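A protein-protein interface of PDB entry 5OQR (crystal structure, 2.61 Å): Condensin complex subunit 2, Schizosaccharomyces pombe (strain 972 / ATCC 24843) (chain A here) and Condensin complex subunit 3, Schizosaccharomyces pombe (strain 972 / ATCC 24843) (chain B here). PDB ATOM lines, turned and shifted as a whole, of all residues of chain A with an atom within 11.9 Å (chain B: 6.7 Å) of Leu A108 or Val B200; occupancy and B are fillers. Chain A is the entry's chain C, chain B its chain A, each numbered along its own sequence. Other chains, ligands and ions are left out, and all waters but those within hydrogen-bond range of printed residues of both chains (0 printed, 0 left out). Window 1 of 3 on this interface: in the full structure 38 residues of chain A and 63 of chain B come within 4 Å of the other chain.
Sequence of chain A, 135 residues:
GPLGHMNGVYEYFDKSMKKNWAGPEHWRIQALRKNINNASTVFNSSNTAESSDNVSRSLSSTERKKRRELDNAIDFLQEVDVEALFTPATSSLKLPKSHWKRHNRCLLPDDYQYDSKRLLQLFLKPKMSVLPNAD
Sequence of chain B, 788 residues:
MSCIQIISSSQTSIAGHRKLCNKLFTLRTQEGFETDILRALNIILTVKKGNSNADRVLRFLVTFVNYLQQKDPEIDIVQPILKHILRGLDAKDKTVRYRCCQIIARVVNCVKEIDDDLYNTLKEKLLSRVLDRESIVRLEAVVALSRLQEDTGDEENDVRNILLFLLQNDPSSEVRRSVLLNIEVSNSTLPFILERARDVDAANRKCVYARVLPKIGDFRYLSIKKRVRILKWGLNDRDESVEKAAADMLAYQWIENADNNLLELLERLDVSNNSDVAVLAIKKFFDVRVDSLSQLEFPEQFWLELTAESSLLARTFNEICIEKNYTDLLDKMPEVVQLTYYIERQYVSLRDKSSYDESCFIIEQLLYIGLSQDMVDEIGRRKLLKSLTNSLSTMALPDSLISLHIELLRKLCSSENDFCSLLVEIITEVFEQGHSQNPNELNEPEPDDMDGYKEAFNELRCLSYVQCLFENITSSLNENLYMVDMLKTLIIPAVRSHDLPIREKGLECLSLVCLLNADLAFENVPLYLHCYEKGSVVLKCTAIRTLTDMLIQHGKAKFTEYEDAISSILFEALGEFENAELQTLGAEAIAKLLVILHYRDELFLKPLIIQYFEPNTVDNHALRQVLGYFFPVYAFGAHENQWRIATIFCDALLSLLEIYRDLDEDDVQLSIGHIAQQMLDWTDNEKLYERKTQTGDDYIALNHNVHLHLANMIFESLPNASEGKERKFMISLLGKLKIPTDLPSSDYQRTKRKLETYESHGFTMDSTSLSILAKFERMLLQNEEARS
CA of Asp B199 touches O of Cys A106 (3.9 Å). Cys A106 touches Val B200 (C to CG2, 3.2 Å). CD2 of Leu A107 touches NH2 of Arg B196 (3.98 Å). Arg B198 touches Leu A107. Asp B199 touches Leu A107 (N to CD2, 3.8 Å). Val B200 touches Leu A107. Val B200 touches Leu A108. Leu A108 touches Arg B205. CD2 of Tyr A112 touches NH1 of Arg B198, 3.6 Å away. Tyr A112 touches Arg B238.
Along chain A the printed residues that touch a printed residue of chain B span positions 106 to 112. Of the 13 printed residues of chain B, 7 touch a printed residue of chain A.
The guanidinium group (NH2) of Arg B176 lies within hydrogen-bond range of the side-chain sulfur (SG) of Cys A106. The guanidinium group of Arg B196 lies within hydrogen-bond range of the backbone carbonyl oxygen of Cys A106. O of Arg B198 is in hydrogen-bond range of N of Leu A108 (3.0 Å). NH1 of Arg B198 sits at hydrogen-bond distance from O of Pro A109 (3.4 Å). NH2 of Arg B238 is in hydrogen-bond range of O of Asp A111 (3.1 Å).
The guanidinium group (NE) of Arg B176 lies within salt-bridge range of the side-chain carboxylate (OD1) of Asp B199. The side-chain carboxylate (OD2) of Asp B199 lies within hydrogen-bond range of the backbone NH (N) of Asp B201, at 2.7 Å. The backbone carbonyl oxygen (O) of Asp B199 sits at hydrogen-bond distance from the guanidinium group (NE) of Arg B205 (2.6 Å). The backbone carbonyl oxygen of Val B200 is in hydrogen-bond range of the guanidinium group of Arg B205 (3.3 Å). NH2 of Arg B205 is in salt-bridge range of OD1 of Asp B237 (2.8 Å). The side-chain amide nitrogen (NE2) of Gln A113 lies close to the side-chain hydroxyl (OH) of Tyr A112 (3.3 Å).
Printed residues of chain B within 4 Å of Leu A107: Arg B196, Arg B198, Asp B199 and Val B200. Leu A108 touches four residues of chain B. Printed residues of chain B within 4 Å of Pro A109: Arg B198. Of the printed residues of chain B, Asp A111 touches Arg B238. Printed residues of chain A within 4 Å of Arg B176: Cys A106 (3.4 Å). Of chain A, only Leu A107 (3.3 Å), Leu A108 (3.0 Å), Pro A109 (3.4 Å) and Tyr A112 (3.6 Å) come within 4 Å of Arg B198. Asp B199 touches just these residues of chain A: Cys A106 (3.9 Å), Leu A107 (3.8 Å) and Leu A108 (3.5 Å). Of the printed residues of chain A, Val B200 touches Cys A106, Leu A107 and Leu A108. No residue of chain A comes within 4 Å of Asp B201. No residue of chain A comes within 4 Å of Ala B202. Of the printed residues of chain A, Arg B238 touches Asp A111 (3.1 Å) and Tyr A112 (3.8 Å). The nearest residue of chain B that does not touch Leu A108 is Asp B237 (5.0 Å). The nearest printed residue of chain B that does not touch Cys A106 is Arg B198 (4.5 Å).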
ATOM      1  N   HIS A 103      12.152  39.284  28.020  1.00  0.00           N
ATOM      2  CA  HIS A 103      11.645  38.884  26.712  1.00  0.00           C
ATOM      3  C   HIS A 103      11.560  37.366  26.617  1.00  0.00           C
ATOM      4  O   HIS A 103      12.409  36.660  27.160  1.00  0.00           O
ATOM      5  CB  HIS A 103      12.539  39.432  25.600  1.00  0.00           C
ATOM      6  CG  HIS A 103      13.917  38.847  25.588  1.00  0.00           C
ATOM      7  ND1 HIS A 103      14.172  37.548  25.204  1.00  0.00           N
ATOM      8  CD2 HIS A 103      15.117  39.384  25.912  1.00  0.00           C
ATOM      9  CE1 HIS A 103      15.469  37.310  25.293  1.00  0.00           C
ATOM     10  NE2 HIS A 103      16.065  38.409  25.719  1.00  0.00           N
ATOM     11  N   ASN A 104      10.540  36.868  25.918  1.00  0.00           N
ATOM     12  CA  ASN A 104      10.296  35.431  25.822  1.00  0.00           C
ATOM     13  C   ASN A 104      10.362  34.802  27.211  1.00  0.00           C
ATOM     14  O   ASN A 104      11.062  33.817  27.444  1.00  0.00           O
ATOM     15  CB  ASN A 104      11.300  34.771  24.874  1.00  0.00           C
ATOM     16  CG  ASN A 104      11.548  35.591  23.621  1.00  0.00           C
ATOM     17  OD1 ASN A 104      10.970  36.663  23.442  1.00  0.00           O
ATOM     18  ND2 ASN A 104      12.425  35.095  22.755  1.00  0.00           N
ATOM     19  N   ARG A 105       9.614  35.393  28.144  1.00  0.00           N
ATOM     20  CA  ARG A 105       9.845  35.183  29.569  1.00  0.00           C
ATOM     21  C   ARG A 105       9.790  33.717  29.981  1.00  0.00           C
ATOM     22  O   ARG A 105       8.949  33.323  30.795  1.00  0.00           O
ATOM     23  CB  ARG A 105       8.839  35.989  30.393  1.00  0.00           C
ATOM     24  CG  ARG A 105       7.374  35.654  30.158  1.00  0.00           C
ATOM     25  CD  ARG A 105       6.562  36.115  31.352  1.00  0.00           C
ATOM     26  NE  ARG A 105       5.127  36.142  31.098  1.00  0.00           N
ATOM     27  CZ  ARG A 105       4.244  36.726  31.900  1.00  0.00           C
ATOM     28  NH1 ARG A 105       4.651  37.338  33.003  1.00  0.00           N
ATOM     29  NH2 ARG A 105       2.953  36.709  31.603  1.00  0.00           N
ATOM     30  N   CYS A 106      10.705  32.913  29.448  1.00  0.00           N
ATOM     31  CA  CYS A 106      10.864  31.519  29.844  1.00  0.00           C
ATOM     32  C   CYS A 106       9.516  30.797  29.877  1.00  0.00           C
ATOM     33  O   CYS A 106       9.028  30.357  30.919  1.00  0.00           O
ATOM     34  CB  CYS A 106      11.581  31.434  31.191  1.00  0.00           C
ATOM     35  SG  CYS A 106      13.192  32.259  31.175  1.00  0.00           S
ATOM     36  N   LEU A 107       8.923  30.680  28.691  1.00  0.00           N
ATOM     37  CA  LEU A 107       7.723  29.883  28.492  1.00  0.00           C
ATOM     38  C   LEU A 107       7.765  29.305  27.087  1.00  0.00           C
ATOM     39  O   LEU A 107       8.270  29.938  26.156  1.00  0.00           O
ATOM     40  CB  LEU A 107       6.448  30.709  28.698  1.00  0.00           C
ATOM     41  CG  LEU A 107       6.165  31.135  30.138  1.00  0.00           C
ATOM     42  CD1 LEU A 107       5.076  32.186  30.177  1.00  0.00           C
ATOM     43  CD2 LEU A 107       5.776  29.932  30.984  1.00  0.00           C
ATOM     44  N   LEU A 108       7.240  28.091  26.947  1.00  0.00           N
ATOM     45  CA  LEU A 108       7.297  27.403  25.672  1.00  0.00           C
ATOM     46  C   LEU A 108       6.519  28.181  24.612  1.00  0.00           C
ATOM     47  O   LEU A 108       5.636  28.979  24.935  1.00  0.00           O
ATOM     48  CB  LEU A 108       6.720  25.997  25.799  1.00  0.00           C
ATOM     49  CG  LEU A 108       7.464  25.045  26.730  1.00  0.00           C
ATOM     50  CD1 LEU A 108       6.577  23.863  27.056  1.00  0.00           C
ATOM     51  CD2 LEU A 108       8.768  24.584  26.097  1.00  0.00           C
ATOM     52  N   PRO A 109       6.829  27.959  23.337  1.00  0.00           N
ATOM     53  CA  PRO A 109       5.997  28.531  22.276  1.00  0.00           C
ATOM     54  C   PRO A 109       4.599  27.937  22.306  1.00  0.00           C
ATOM     55  O   PRO A 109       4.370  26.832  22.803  1.00  0.00           O
ATOM     56  CB  PRO A 109       6.737  28.142  20.990  1.00  0.00           C
ATOM     57  CG  PRO A 109       7.549  26.951  21.368  1.00  0.00           C
ATOM     58  CD  PRO A 109       7.952  27.178  22.791  1.00  0.00           C
ATOM     59  N   ASP A 110       3.650  28.695  21.767  1.00  0.00           N
ATOM     60  CA  ASP A 110       2.299  28.183  21.565  1.00  0.00           C
ATOM     61  C   ASP A 110       2.354  27.262  20.355  1.00  0.00           C
ATOM     62  O   ASP A 110       2.451  27.720  19.216  1.00  0.00           O
ATOM     63  CB  ASP A 110       1.305  29.320  21.360  1.00  0.00           C
ATOM     64  CG  ASP A 110       1.590  30.513  22.248  1.00  0.00           C
ATOM     65  OD1 ASP A 110       1.210  30.476  23.436  1.00  0.00           O
ATOM     66  OD2 ASP A 110       2.190  31.490  21.753  1.00  0.00           O
ATOM     67  N   ASP A 111       2.335  25.952  20.602  1.00  0.00           N
ATOM     68  CA  ASP A 111       2.340  24.972  19.526  1.00  0.00           C
ATOM     69  C   ASP A 111       1.430  23.782  19.792  1.00  0.00           C
ATOM     70  O   ASP A 111       1.290  22.930  18.910  1.00  0.00           O
ATOM     71  CB  ASP A 111       3.770  24.465  19.265  1.00  0.00           C
ATOM     72  CG  ASP A 111       4.635  25.488  18.551  1.00  0.00           C
ATOM     73  OD1 ASP A 111       4.083  26.317  17.797  1.00  0.00           O
ATOM     74  OD2 ASP A 111       5.869  25.456  18.737  1.00  0.00           O
ATOM     75  N   TYR A 112       0.810  23.693  20.969  1.00  0.00           N
ATOM     76  CA  TYR A 112      -0.095  22.592  21.267  1.00  0.00           C
ATOM     77  C   TYR A 112      -1.497  22.817  20.719  1.00  0.00           C
ATOM     78  O   TYR A 112      -2.281  21.863  20.663  1.00  0.00           O
ATOM     79  CB  TYR A 112      -0.170  22.368  22.782  1.00  0.00           C
ATOM     80  CG  TYR A 112      -0.862  23.481  23.541  1.00  0.00           C
ATOM     81  CD1 TYR A 112      -2.240  23.476  23.717  1.00  0.00           C
ATOM     82  CD2 TYR A 112      -0.137  24.533  24.089  1.00  0.00           C
ATOM     83  CE1 TYR A 112      -2.878  24.487  24.407  1.00  0.00           C
ATOM     84  CE2 TYR A 112      -0.769  25.550  24.785  1.00  0.00           C
ATOM     85  CZ  TYR A 112      -2.138  25.521  24.941  1.00  0.00           C
ATOM     86  OH  TYR A 112      -2.772  26.531  25.630  1.00  0.00           O
ATOM     87  N   GLN A 113      -1.830  24.043  20.311  1.00  0.00           N
ATOM     88  CA  GLN A 113      -3.189  24.333  19.868  1.00  0.00           C
ATOM     89  C   GLN A 113      -3.415  23.870  18.436  1.00  0.00           C
ATOM     90  O   GLN A 113      -4.451  23.266  18.134  1.00  0.00           O
ATOM     91  CB  GLN A 113      -3.489  25.828  19.989  1.00  0.00           C
ATOM     92  CG  GLN A 113      -3.401  26.393  21.407  1.00  0.00           C
ATOM     93  CD  GLN A 113      -1.978  26.498  21.912  1.00  0.00           C
ATOM     94  OE1 GLN A 113      -1.140  25.647  21.618  1.00  0.00           O
ATOM     95  NE2 GLN A 113      -1.686  27.562  22.653  1.00  0.00           N
ATOM     96  N   ARG B 176      14.218  29.628  39.251  1.00  0.00           N
ATOM     97  CA  ARG B 176      12.761  29.594  39.190  1.00  0.00           C
ATOM     98  C   ARG B 176      12.208  28.409  39.972  1.00  0.00           C
ATOM     99  O   ARG B 176      11.247  28.547  40.736  1.00  0.00           O
ATOM    100  CB  ARG B 176      12.299  29.534  37.734  1.00  0.00           C
ATOM    101  CG  ARG B 176      12.556  30.805  36.950  1.00  0.00           C
ATOM    102  CD  ARG B 176      11.758  30.834  35.655  1.00  0.00           C
ATOM    103  NE  ARG B 176      12.098  29.730  34.761  1.00  0.00           N
ATOM    104  CZ  ARG B 176      13.195  29.681  34.013  1.00  0.00           C
ATOM    105  NH1 ARG B 176      13.418  28.638  33.226  1.00  0.00           N
ATOM    106  NH2 ARG B 176      14.079  30.666  34.060  1.00  0.00           N
ATOM    107  N   ARG B 196       3.913  28.371  35.304  1.00  0.00           N
ATOM    108  CA  ARG B 196       5.109  27.545  35.199  1.00  0.00           C
ATOM    109  C   ARG B 196       4.808  26.186  34.587  1.00  0.00           C
ATOM    110  O   ARG B 196       5.728  25.523  34.099  1.00  0.00           O
ATOM    111  CB  ARG B 196       5.754  27.353  36.572  1.00  0.00           C
ATOM    112  CG  ARG B 196       5.937  28.622  37.392  1.00  0.00           C
ATOM    113  CD  ARG B 196       6.249  29.858  36.557  1.00  0.00           C
ATOM    114  NE  ARG B 196       7.311  29.641  35.580  1.00  0.00           N
ATOM    115  CZ  ARG B 196       7.622  30.502  34.617  1.00  0.00           C
ATOM    116  NH1 ARG B 196       6.952  31.640  34.499  1.00  0.00           N
ATOM    117  NH2 ARG B 196       8.601  30.226  33.769  1.00  0.00           N
ATOM    118  N   ALA B 197       3.545  25.757  34.600  1.00  0.00           N
ATOM    119  CA  ALA B 197       3.170  24.542  33.892  1.00  0.00           C
ATOM    120  C   ALA B 197       3.525  24.607  32.414  1.00  0.00           C
ATOM    121  O   ALA B 197       3.488  23.573  31.741  1.00  0.00           O
ATOM    122  CB  ALA B 197       1.674  24.278  34.060  1.00  0.00           C
ATOM    123  N   ARG B 198       3.858  25.791  31.896  1.00  0.00           N
ATOM    124  CA  ARG B 198       4.387  25.942  30.546  1.00  0.00           C
ATOM    125  C   ARG B 198       5.817  26.471  30.556  1.00  0.00           C
ATOM    126  O   ARG B 198       6.269  27.047  29.561  1.00  0.00           O
ATOM    127  CB  ARG B 198       3.486  26.860  29.717  1.00  0.00           C
ATOM    128  CG  ARG B 198       2.095  26.303  29.460  1.00  0.00           C
ATOM    129  CD  ARG B 198       2.137  25.038  28.613  1.00  0.00           C
ATOM    130  NE  ARG B 198       2.604  25.297  27.254  1.00  0.00           N
ATOM    131  CZ  ARG B 198       2.863  24.348  26.360  1.00  0.00           C
ATOM    132  NH1 ARG B 198       3.278  24.678  25.145  1.00  0.00           N
ATOM    133  NH2 ARG B 198       2.712  23.069  26.678  1.00  0.00           N
ATOM    134  N   ASP B 199       6.534  26.287  31.660  1.00  0.00           N
ATOM    135  CA  ASP B 199       7.934  26.676  31.718  1.00  0.00           C
ATOM    136  C   ASP B 199       8.720  25.968  30.621  1.00  0.00           C
ATOM    137  O   ASP B 199       8.350  24.885  30.161  1.00  0.00           O
ATOM    138  CB  ASP B 199       8.521  26.338  33.087  1.00  0.00           C
ATOM    139  CG  ASP B 199       9.872  26.982  33.320  1.00  0.00           C
ATOM    140  OD1 ASP B 199       9.918  28.049  33.968  1.00  0.00           O
ATOM    141  OD2 ASP B 199      10.888  26.424  32.856  1.00  0.00           O
ATOM    142  N   VAL B 200       9.822  26.592  30.199  1.00  0.00           N
ATOM    143  CA  VAL B 200      10.615  26.019  29.116  1.00  0.00           C
ATOM    144  C   VAL B 200      11.319  24.757  29.589  1.00  0.00           C
ATOM    145  O   VAL B 200      11.604  23.858  28.789  1.00  0.00           O
ATOM    146  CB  VAL B 200      11.636  27.034  28.566  1.00  0.00           C
ATOM    147  CG1 VAL B 200      12.181  26.558  27.232  1.00  0.00           C
ATOM    148  CG2 VAL B 200      11.026  28.408  28.428  1.00  0.00           C
ATOM    149  N   ASP B 201      11.616  24.670  30.881  1.00  0.00           N
ATOM    150  CA  ASP B 201      12.326  23.530  31.440  1.00  0.00           C
ATOM    151  C   ASP B 201      11.325  22.473  31.890  1.00  0.00           C
ATOM    152  O   ASP B 201      10.371  22.778  32.613  1.00  0.00           O
ATOM    153  CB  ASP B 201      13.203  23.967  32.612  1.00  0.00           C
ATOM    154  CG  ASP B 201      13.949  22.811  33.243  1.00  0.00           C
ATOM    155  OD1 ASP B 201      13.404  22.205  34.186  1.00  0.00           O
ATOM    156  OD2 ASP B 201      15.075  22.506  32.796  1.00  0.00           O
ATOM    157  N   ALA B 202      11.550  21.231  31.458  1.00  0.00           N
ATOM    158  CA  ALA B 202      10.623  20.153  31.787  1.00  0.00           C
ATOM    159  C   ALA B 202      10.541  19.931  33.292  1.00  0.00           C
ATOM    160  O   ALA B 202       9.453  19.703  33.833  1.00  0.00           O
ATOM    161  CB  ALA B 202      11.048  18.867  31.081  1.00  0.00           C
ATOM    162  N   ALA B 203      11.680  19.990  33.986  1.00  0.00           N
ATOM    163  CA  ALA B 203      11.674  19.744  35.424  1.00  0.00           C
ATOM    164  C   ALA B 203      10.808  20.762  36.152  1.00  0.00           C
ATOM    165  O   ALA B 203      10.106  20.418  37.109  1.00  0.00           O
ATOM    166  CB  ALA B 203      13.102  19.760  35.972  1.00  0.00           C
ATOM    167  N   ASN B 204      10.840  22.021  35.713  1.00  0.00           N
ATOM    168  CA  ASN B 204       9.996  23.034  36.337  1.00  0.00           C
ATOM    169  C   ASN B 204       8.522  22.740  36.100  1.00  0.00           C
ATOM    170  O   ASN B 204       7.702  22.868  37.016  1.00  0.00           O
ATOM    171  CB  ASN B 204      10.356  24.420  35.806  1.00  0.00           C
ATOM    172  CG  ASN B 204      11.788  24.801  36.105  1.00  0.00           C
ATOM    173  OD1 ASN B 204      12.694  23.971  36.023  1.00  0.00           O
ATOM    174  ND2 ASN B 204      12.003  26.060  36.465  1.00  0.00           N
ATOM    175  N   ARG B 205       8.165  22.349  34.876  1.00  0.00           N
ATOM    176  CA  ARG B 205       6.790  21.951  34.595  1.00  0.00           C
ATOM    177  C   ARG B 205       6.372  20.789  35.484  1.00  0.00           C
ATOM    178  O   ARG B 205       5.317  20.828  36.125  1.00  0.00           O
ATOM    179  CB  ARG B 205       6.648  21.572  33.122  1.00  0.00           C
ATOM    180  CG  ARG B 205       6.584  22.755  32.181  1.00  0.00           C
ATOM    181  CD  ARG B 205       6.355  22.313  30.748  1.00  0.00           C
ATOM    182  NE  ARG B 205       7.579  22.402  29.950  1.00  0.00           N
ATOM    183  CZ  ARG B 205       8.117  21.412  29.242  1.00  0.00           C
ATOM    184  NH1 ARG B 205       9.232  21.629  28.557  1.00  0.00           N
ATOM    185  NH2 ARG B 205       7.551  20.215  29.193  1.00  0.00           N
ATOM    186  N   ASP B 237       1.365  17.357  27.526  1.00  0.00           N
ATOM    187  CA  ASP B 237       2.724  17.873  27.555  1.00  0.00           C
ATOM    188  C   ASP B 237       3.646  17.034  26.675  1.00  0.00           C
ATOM    189  O   ASP B 237       3.463  15.826  26.511  1.00  0.00           O
ATOM    190  CB  ASP B 237       3.254  17.899  28.985  1.00  0.00           C
ATOM    191  CG  ASP B 237       4.524  18.713  29.118  1.00  0.00           C
ATOM    192  OD1 ASP B 237       5.620  18.139  28.952  1.00  0.00           O
ATOM    193  OD2 ASP B 237       4.425  19.931  29.376  1.00  0.00           O
ATOM    194  N   ARG B 238       4.657  17.698  26.114  1.00  0.00           N
ATOM    195  CA  ARG B 238       5.563  17.039  25.180  1.00  0.00           C
ATOM    196  C   ARG B 238       6.533  16.106  25.893  1.00  0.00           C
ATOM    197  O   ARG B 238       7.001  15.130  25.296  1.00  0.00           O
ATOM    198  CB  ARG B 238       6.339  18.087  24.385  1.00  0.00           C
ATOM    199  CG  ARG B 238       5.465  19.116  23.686  1.00  0.00           C
ATOM    200  CD  ARG B 238       4.898  18.576  22.387  1.00  0.00           C
ATOM    201  NE  ARG B 238       3.975  19.522  21.766  1.00  0.00           N
ATOM    202  CZ  ARG B 238       3.593  19.477  20.494  1.00  0.00           C
ATOM    203  NH1 ARG B 238       4.060  18.533  19.686  1.00  0.00           N
ATOM    204  NH2 ARG B 238       2.747  20.382  20.024  1.00  0.00           N
